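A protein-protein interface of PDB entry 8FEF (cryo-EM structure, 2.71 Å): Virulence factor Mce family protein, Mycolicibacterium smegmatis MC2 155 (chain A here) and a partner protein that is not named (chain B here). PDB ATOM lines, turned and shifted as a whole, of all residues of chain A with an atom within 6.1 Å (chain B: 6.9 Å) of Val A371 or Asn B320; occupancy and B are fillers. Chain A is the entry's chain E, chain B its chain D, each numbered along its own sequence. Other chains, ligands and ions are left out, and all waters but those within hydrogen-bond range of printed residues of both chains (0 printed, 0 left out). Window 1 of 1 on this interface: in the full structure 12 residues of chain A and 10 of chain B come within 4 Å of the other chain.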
ATOM      1  N   ASN A 341      -8.525   8.677 -15.112  1.00  0.00           N
ATOM      2  CA  ASN A 341      -8.652   7.611 -14.123  1.00  0.00           C
ATOM      3  C   ASN A 341      -9.018   8.152 -12.747  1.00  0.00           C
ATOM      4  O   ASN A 341      -9.757   7.498 -12.005  1.00  0.00           O
ATOM      5  CB  ASN A 341      -7.363   6.795 -14.047  1.00  0.00           C
ATOM      6  CG  ASN A 341      -7.565   5.353 -14.468  1.00  0.00           C
ATOM      7  OD1 ASN A 341      -8.692   4.914 -14.689  1.00  0.00           O
ATOM      8  ND2 ASN A 341      -6.476   4.605 -14.572  1.00  0.00           N
ATOM      9  N   SER A 345     -13.765   8.238 -13.949  1.00  0.00           N
ATOM     10  CA  SER A 345     -14.063   6.813 -13.965  1.00  0.00           C
ATOM     11  C   SER A 345     -15.437   6.565 -13.360  1.00  0.00           C
ATOM     12  O   SER A 345     -15.823   7.202 -12.376  1.00  0.00           O
ATOM     13  CB  SER A 345     -13.003   6.026 -13.195  1.00  0.00           C
ATOM     14  OG  SER A 345     -11.766   6.025 -13.883  1.00  0.00           O
ATOM     15  N   GLY A 346     -16.181   5.641 -13.958  1.00  0.00           N
ATOM     16  CA  GLY A 346     -17.516   5.348 -13.487  1.00  0.00           C
ATOM     17  C   GLY A 346     -18.568   6.358 -13.876  1.00  0.00           C
ATOM     18  O   GLY A 346     -19.675   6.317 -13.327  1.00  0.00           O
ATOM     19  N   SER A 350     -15.975   9.119 -19.405  1.00  0.00           N
ATOM     20  CA  SER A 350     -14.727   8.394 -19.188  1.00  0.00           C
ATOM     21  C   SER A 350     -13.765   8.569 -20.358  1.00  0.00           C
ATOM     22  O   SER A 350     -12.564   8.779 -20.158  1.00  0.00           O
ATOM     23  CB  SER A 350     -15.020   6.914 -18.949  1.00  0.00           C
ATOM     24  OG  SER A 350     -13.838   6.208 -18.615  1.00  0.00           O
ATOM     25  N   ILE A 368      -1.558   4.780 -17.897  1.00  0.00           N
ATOM     26  CA  ILE A 368      -2.204   4.004 -16.834  1.00  0.00           C
ATOM     27  C   ILE A 368      -3.342   3.194 -17.450  1.00  0.00           C
ATOM     28  O   ILE A 368      -4.018   3.691 -18.375  1.00  0.00           O
ATOM     29  CB  ILE A 368      -2.703   4.941 -15.713  1.00  0.00           C
ATOM     30  CG1 ILE A 368      -3.143   4.167 -14.469  1.00  0.00           C
ATOM     31  CG2 ILE A 368      -3.801   5.879 -16.203  1.00  0.00           C
ATOM     32  CD1 ILE A 368      -3.319   5.034 -13.247  1.00  0.00           C
ATOM     33  N   PRO A 369      -3.541   1.931 -17.065  1.00  0.00           N
ATOM     34  CA  PRO A 369      -4.477   1.073 -17.803  1.00  0.00           C
ATOM     35  C   PRO A 369      -5.892   1.630 -17.839  1.00  0.00           C
ATOM     36  O   PRO A 369      -6.380   2.213 -16.871  1.00  0.00           O
ATOM     37  CB  PRO A 369      -4.412  -0.252 -17.039  1.00  0.00           C
ATOM     38  CG  PRO A 369      -3.051  -0.263 -16.467  1.00  0.00           C
ATOM     39  CD  PRO A 369      -2.756   1.153 -16.091  1.00  0.00           C
ATOM     40  N   ASP A 370      -6.545   1.445 -18.984  1.00  0.00           N
ATOM     41  CA  ASP A 370      -7.914   1.907 -19.191  1.00  0.00           C
ATOM     42  C   ASP A 370      -8.857   0.874 -18.594  1.00  0.00           C
ATOM     43  O   ASP A 370      -9.115  -0.169 -19.198  1.00  0.00           O
ATOM     44  CB  ASP A 370      -8.189   2.124 -20.674  1.00  0.00           C
ATOM     45  CG  ASP A 370      -7.207   3.087 -21.316  1.00  0.00           C
ATOM     46  OD1 ASP A 370      -6.280   3.550 -20.617  1.00  0.00           O
ATOM     47  OD2 ASP A 370      -7.359   3.382 -22.519  1.00  0.00           O
ATOM     48  N   VAL A 371      -9.391   1.177 -17.408  1.00  0.00           N
ATOM     49  CA  VAL A 371     -10.179   0.226 -16.633  1.00  0.00           C
ATOM     50  C   VAL A 371     -11.451  -0.219 -17.340  1.00  0.00           C
ATOM     51  O   VAL A 371     -12.076  -1.194 -16.914  1.00  0.00           O
ATOM     52  CB  VAL A 371     -10.527   0.831 -15.256  1.00  0.00           C
ATOM     53  CG1 VAL A 371      -9.278   0.964 -14.408  1.00  0.00           C
ATOM     54  CG2 VAL A 371     -11.201   2.181 -15.428  1.00  0.00           C
ATOM     55  N   ARG A 372     -11.854   0.473 -18.407  1.00  0.00           N
ATOM     56  CA  ARG A 372     -13.086   0.123 -19.099  1.00  0.00           C
ATOM     57  C   ARG A 372     -12.985  -1.207 -19.830  1.00  0.00           C
ATOM     58  O   ARG A 372     -14.014  -1.846 -20.071  1.00  0.00           O
ATOM     59  CB  ARG A 372     -13.465   1.226 -20.088  1.00  0.00           C
ATOM     60  CG  ARG A 372     -13.668   2.588 -19.455  1.00  0.00           C
ATOM     61  CD  ARG A 372     -14.336   3.545 -20.426  1.00  0.00           C
ATOM     62  NE  ARG A 372     -13.579   3.691 -21.662  1.00  0.00           N
ATOM     63  CZ  ARG A 372     -13.989   4.385 -22.715  1.00  0.00           C
ATOM     64  NH1 ARG A 372     -15.154   5.012 -22.717  1.00  0.00           N
ATOM     65  NH2 ARG A 372     -13.213   4.450 -23.792  1.00  0.00           N
ATOM     66  N   PHE A 373     -11.777  -1.639 -20.193  1.00  0.00           N
ATOM     67  CA  PHE A 373     -11.615  -2.797 -21.063  1.00  0.00           C
ATOM     68  C   PHE A 373     -10.634  -3.846 -20.562  1.00  0.00           C
ATOM     69  O   PHE A 373     -10.766  -5.008 -20.962  1.00  0.00           O
ATOM     70  CB  PHE A 373     -11.179  -2.353 -22.466  1.00  0.00           C
ATOM     71  CG  PHE A 373     -12.106  -1.356 -23.100  1.00  0.00           C
ATOM     72  CD1 PHE A 373     -13.267  -1.773 -23.730  1.00  0.00           C
ATOM     73  CD2 PHE A 373     -11.815  -0.003 -23.070  1.00  0.00           C
ATOM     74  CE1 PHE A 373     -14.120  -0.858 -24.314  1.00  0.00           C
ATOM     75  CE2 PHE A 373     -12.666   0.916 -23.651  1.00  0.00           C
ATOM     76  CZ  PHE A 373     -13.819   0.488 -24.273  1.00  0.00           C
ATOM     77  N   THR A 374      -9.664  -3.496 -19.723  1.00  0.00           N
ATOM     78  CA  THR A 374      -8.673  -4.480 -19.289  1.00  0.00           C
ATOM     79  C   THR A 374      -9.320  -5.499 -18.356  1.00  0.00           C
ATOM     80  O   THR A 374      -9.830  -5.120 -17.294  1.00  0.00           O
ATOM     81  CB  THR A 374      -7.482  -3.792 -18.615  1.00  0.00           C
ATOM     82  OG1 THR A 374      -6.697  -4.763 -17.913  1.00  0.00           O
ATOM     83  CG2 THR A 374      -7.929  -2.702 -17.653  1.00  0.00           C
ATOM     84  N   ASN B 317      -6.491   1.303  -0.685  1.00  0.00           N
ATOM     85  CA  ASN B 317      -6.058   0.978  -2.038  1.00  0.00           C
ATOM     86  C   ASN B 317      -7.246   1.107  -2.980  1.00  0.00           C
ATOM     87  O   ASN B 317      -8.187   0.309  -2.915  1.00  0.00           O
ATOM     88  CB  ASN B 317      -5.481  -0.433  -2.081  1.00  0.00           C
ATOM     89  CG  ASN B 317      -4.394  -0.647  -1.053  1.00  0.00           C
ATOM     90  OD1 ASN B 317      -3.502   0.182  -0.896  1.00  0.00           O
ATOM     91  ND2 ASN B 317      -4.465  -1.764  -0.340  1.00  0.00           N
ATOM     92  N   SER B 318      -7.203   2.110  -3.857  1.00  0.00           N
ATOM     93  CA  SER B 318      -8.257   2.315  -4.837  1.00  0.00           C
ATOM     94  C   SER B 318      -7.937   1.509  -6.088  1.00  0.00           C
ATOM     95  O   SER B 318      -6.929   1.794  -6.750  1.00  0.00           O
ATOM     96  CB  SER B 318      -8.394   3.790  -5.175  1.00  0.00           C
ATOM     97  OG  SER B 318      -7.130   4.365  -5.446  1.00  0.00           O
ATOM     98  N   PRO B 319      -8.731   0.493  -6.433  1.00  0.00           N
ATOM     99  CA  PRO B 319      -8.393  -0.337  -7.603  1.00  0.00           C
ATOM    100  C   PRO B 319      -8.339   0.428  -8.917  1.00  0.00           C
ATOM    101  O   PRO B 319      -7.496   0.120  -9.767  1.00  0.00           O
ATOM    102  CB  PRO B 319      -9.506  -1.393  -7.608  1.00  0.00           C
ATOM    103  CG  PRO B 319      -9.998  -1.434  -6.207  1.00  0.00           C
ATOM    104  CD  PRO B 319      -9.888  -0.036  -5.695  1.00  0.00           C
ATOM    105  N   ASN B 320      -9.216   1.416  -9.110  1.00  0.00           N
ATOM    106  CA  ASN B 320      -9.305   2.088 -10.404  1.00  0.00           C
ATOM    107  C   ASN B 320      -8.108   2.986 -10.670  1.00  0.00           C
ATOM    108  O   ASN B 320      -7.697   3.138 -11.825  1.00  0.00           O
ATOM    109  CB  ASN B 320     -10.587   2.909 -10.489  1.00  0.00           C
ATOM    110  CG  ASN B 320     -11.819   2.052 -10.562  1.00  0.00           C
ATOM    111  OD1 ASN B 320     -11.737   0.850 -10.806  1.00  0.00           O
ATOM    112  ND2 ASN B 320     -12.977   2.663 -10.358  1.00  0.00           N
ATOM    113  N   GLN B 321      -7.558   3.613  -9.634  1.00  0.00           N
ATOM    114  CA  GLN B 321      -6.415   4.496  -9.796  1.00  0.00           C
ATOM    115  C   GLN B 321      -5.109   3.867  -9.338  1.00  0.00           C
ATOM    116  O   GLN B 321      -4.049   4.467  -9.540  1.00  0.00           O
ATOM    117  CB  GLN B 321      -6.642   5.811  -9.035  1.00  0.00           C
ATOM    118  CG  GLN B 321      -7.859   6.608  -9.481  1.00  0.00           C
ATOM    119  CD  GLN B 321      -9.157   6.089  -8.898  1.00  0.00           C
ATOM    120  OE1 GLN B 321      -9.164   5.436  -7.858  1.00  0.00           O
ATOM    121  NE2 GLN B 321     -10.265   6.373  -9.572  1.00  0.00           N
ATOM    122  N   GLY B 322      -5.156   2.683  -8.730  1.00  0.00           N
ATOM    123  CA  GLY B 322      -3.962   2.022  -8.241  1.00  0.00           C
ATOM    124  C   GLY B 322      -3.307   2.723  -7.070  1.00  0.00           C
ATOM    125  O   GLY B 322      -3.620   3.877  -6.767  1.00  0.00           O
ATOM    126  N   ALA B 388     -14.781   7.813  -7.970  1.00  0.00           N
ATOM    127  CA  ALA B 388     -15.022   6.373  -8.016  1.00  0.00           C
ATOM    128  C   ALA B 388     -13.735   5.621  -7.709  1.00  0.00           C
ATOM    129  O   ALA B 388     -12.822   5.571  -8.539  1.00  0.00           O
ATOM    130  CB  ALA B 388     -15.572   5.973  -9.381  1.00  0.00           C
ATOM    131  N   MET B 389     -13.653   5.039  -6.512  1.00  0.00           N
ATOM    132  CA  MET B 389     -12.517   4.185  -6.186  1.00  0.00           C
ATOM    133  C   MET B 389     -12.615   2.829  -6.871  1.00  0.00           C
ATOM    134  O   MET B 389     -11.612   2.314  -7.374  1.00  0.00           O
ATOM    135  CB  MET B 389     -12.403   4.007  -4.672  1.00  0.00           C
ATOM    136  CG  MET B 389     -12.088   5.282  -3.913  1.00  0.00           C
ATOM    137  SD  MET B 389     -11.683   4.961  -2.188  1.00  0.00           S
ATOM    138  CE  MET B 389     -11.481   6.628  -1.569  1.00  0.00           C
ATOM    139  N   THR B 390     -13.804   2.236  -6.905  1.00  0.00           N
ATOM    140  CA  THR B 390     -14.015   0.923  -7.501  1.00  0.00           C
ATOM    141  C   THR B 390     -15.110   1.002  -8.563  1.00  0.00           C
ATOM    142  O   THR B 390     -15.716   2.050  -8.792  1.00  0.00           O
ATOM    143  CB  THR B 390     -14.385  -0.119  -6.439  1.00  0.00           C
ATOM    144  OG1 THR B 390     -15.768   0.013  -6.098  1.00  0.00           O
ATOM    145  CG2 THR B 390     -13.548   0.055  -5.184  1.00  0.00           C
ATOM    146  N   LEU B 391     -15.352  -0.127  -9.214  1.00  0.00           N
ATOM    147  CA  LEU B 391     -16.388  -0.292 -10.221  1.00  0.00           C
ATOM    148  C   LEU B 391     -17.189  -1.541  -9.894  1.00  0.00           C
ATOM    149  O   LEU B 391     -16.698  -2.431  -9.191  1.00  0.00           O
ATOM    150  CB  LEU B 391     -15.784  -0.407 -11.630  1.00  0.00           C
ATOM    151  CG  LEU B 391     -15.045   0.801 -12.205  1.00  0.00           C
ATOM    152  CD1 LEU B 391     -14.650   0.541 -13.647  1.00  0.00           C
ATOM    153  CD2 LEU B 391     -15.887   2.057 -12.100  1.00  0.00           C
ATOM    154  N   LYS B 393     -17.951  -4.137 -11.645  1.00  0.00           N
ATOM    155  CA  LYS B 393     -17.388  -5.366 -12.188  1.00  0.00           C
ATOM    156  C   LYS B 393     -16.130  -5.823 -11.463  1.00  0.00           C
ATOM    157  O   LYS B 393     -15.658  -6.934 -11.722  1.00  0.00           O
ATOM    158  CB  LYS B 393     -17.072  -5.188 -13.674  1.00  0.00           C
ATOM    159  CG  LYS B 393     -15.965  -4.187 -13.945  1.00  0.00           C
ATOM    160  CD  LYS B 393     -15.734  -4.000 -15.432  1.00  0.00           C
ATOM    161  CE  LYS B 393     -14.671  -2.946 -15.690  1.00  0.00           C
ATOM    162  NZ  LYS B 393     -14.465  -2.712 -17.144  1.00  0.00           N
ATOM    163  N   GLN B 394     -15.577  -5.003 -10.570  1.00  0.00           N
ATOM    164  CA  GLN B 394     -14.331  -5.331  -9.896  1.00  0.00           C
ATOM    165  C   GLN B 394     -14.521  -5.941  -8.516  1.00  0.00           C
ATOM    166  O   GLN B 394     -13.586  -6.559  -7.999  1.00  0.00           O
ATOM    167  CB  GLN B 394     -13.457  -4.081  -9.762  1.00  0.00           C
ATOM    168  CG  GLN B 394     -13.123  -3.415 -11.076  1.00  0.00           C
ATOM    169  CD  GLN B 394     -12.248  -2.200 -10.891  1.00  0.00           C
ATOM    170  OE1 GLN B 394     -11.846  -1.881  -9.774  1.00  0.00           O
ATOM    171  NE2 GLN B 394     -11.947  -1.513 -11.984  1.00  0.00           N
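ND2 of Asn A341 lies within hydrogen-bond range of O of Asn B320 (3.3 Å).
The backbone carbonyl oxygen (O) of Asn A341 is in hydrogen-bond range of the side-chain amide nitrogen (NE2) of Gln B321 (2.7 Å).
O of Val A371 sits at hydrogen-bond distance from NZ of Lys B393 (2.8 Å).
The side-chain amino group (NZ) of Lys B393 lies within hydrogen-bond range of the backbone carbonyl oxygen (O) of Arg A372 (3.1 Å).
OE1 of Gln B321 sits close to OG of Ser B318, 3.3 Å away.
N of Asn B320 sits at hydrogen-bond distance from O of Met B389 (3.1 Å).
The backbone carbonyl oxygen (O) of Thr B390 lies within hydrogen-bond range of the side-chain amide nitrogen (ND2) of Asn B320 (3.2 Å).
The backbone carbonyl oxygen (O) of Ala B388 sits at hydrogen-bond distance from the side-chain amide nitrogen (NE2) of Gln B321, 2.9 Å away.
The side-chain hydroxyl (OG) of Ser A345 is in hydrogen-bond range of the backbone carbonyl oxygen (O) of Asn A341 (3.1 Å).
O of Pro A369 sits at hydrogen-bond distance from ND2 of Asn A341 (3.3 Å).
CB of Ala B388 touches O of Ser A345, at 3.2 Å.
Gly A346 touches Leu B391.
Gln B321 touches Ile A368.
Asn B320 touches Val A371.
Val A371 touches just these residues of chain B: Asn B320 and Lys B393.
Of chain A, only Asn A341 (3.3 Å) and Val A371 (3.7 Å) come within 4 Å of Asn B320.
Printed residues of chain B within 4 Å of Arg A372: Lys B393.
Printed residues of chain B within 4 Å of Gly A346: Leu B391 (3.9 Å).
Of the printed residues of chain B, Ser A345 touches Ala B388 (3.2 Å).
Of the printed residues of chain A, Ala B388 touches Ser A345 (3.2 Å).
Thr B390 touches none of the printed residues of chain A.
Met B389 touches none of the printed residues of chain A.
The nearest residue of chain A that does not touch Asn B320 is Ser A345 (4.4 Å).
Printed residues of chain A that touch a printed residue of chain B: Asn A341, Ser A345, Gly A346, Ile A368, Val A371 and Arg A372.
Hydrophobic or aromatic side chains of chain A within 4 Å of the printed part of chain B: Ile A368 and Val A371.
Among the printed residues, no Asp or Glu carboxylate lies within 4 Å of a Lys or Arg side-chain nitrogen of the other chain.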
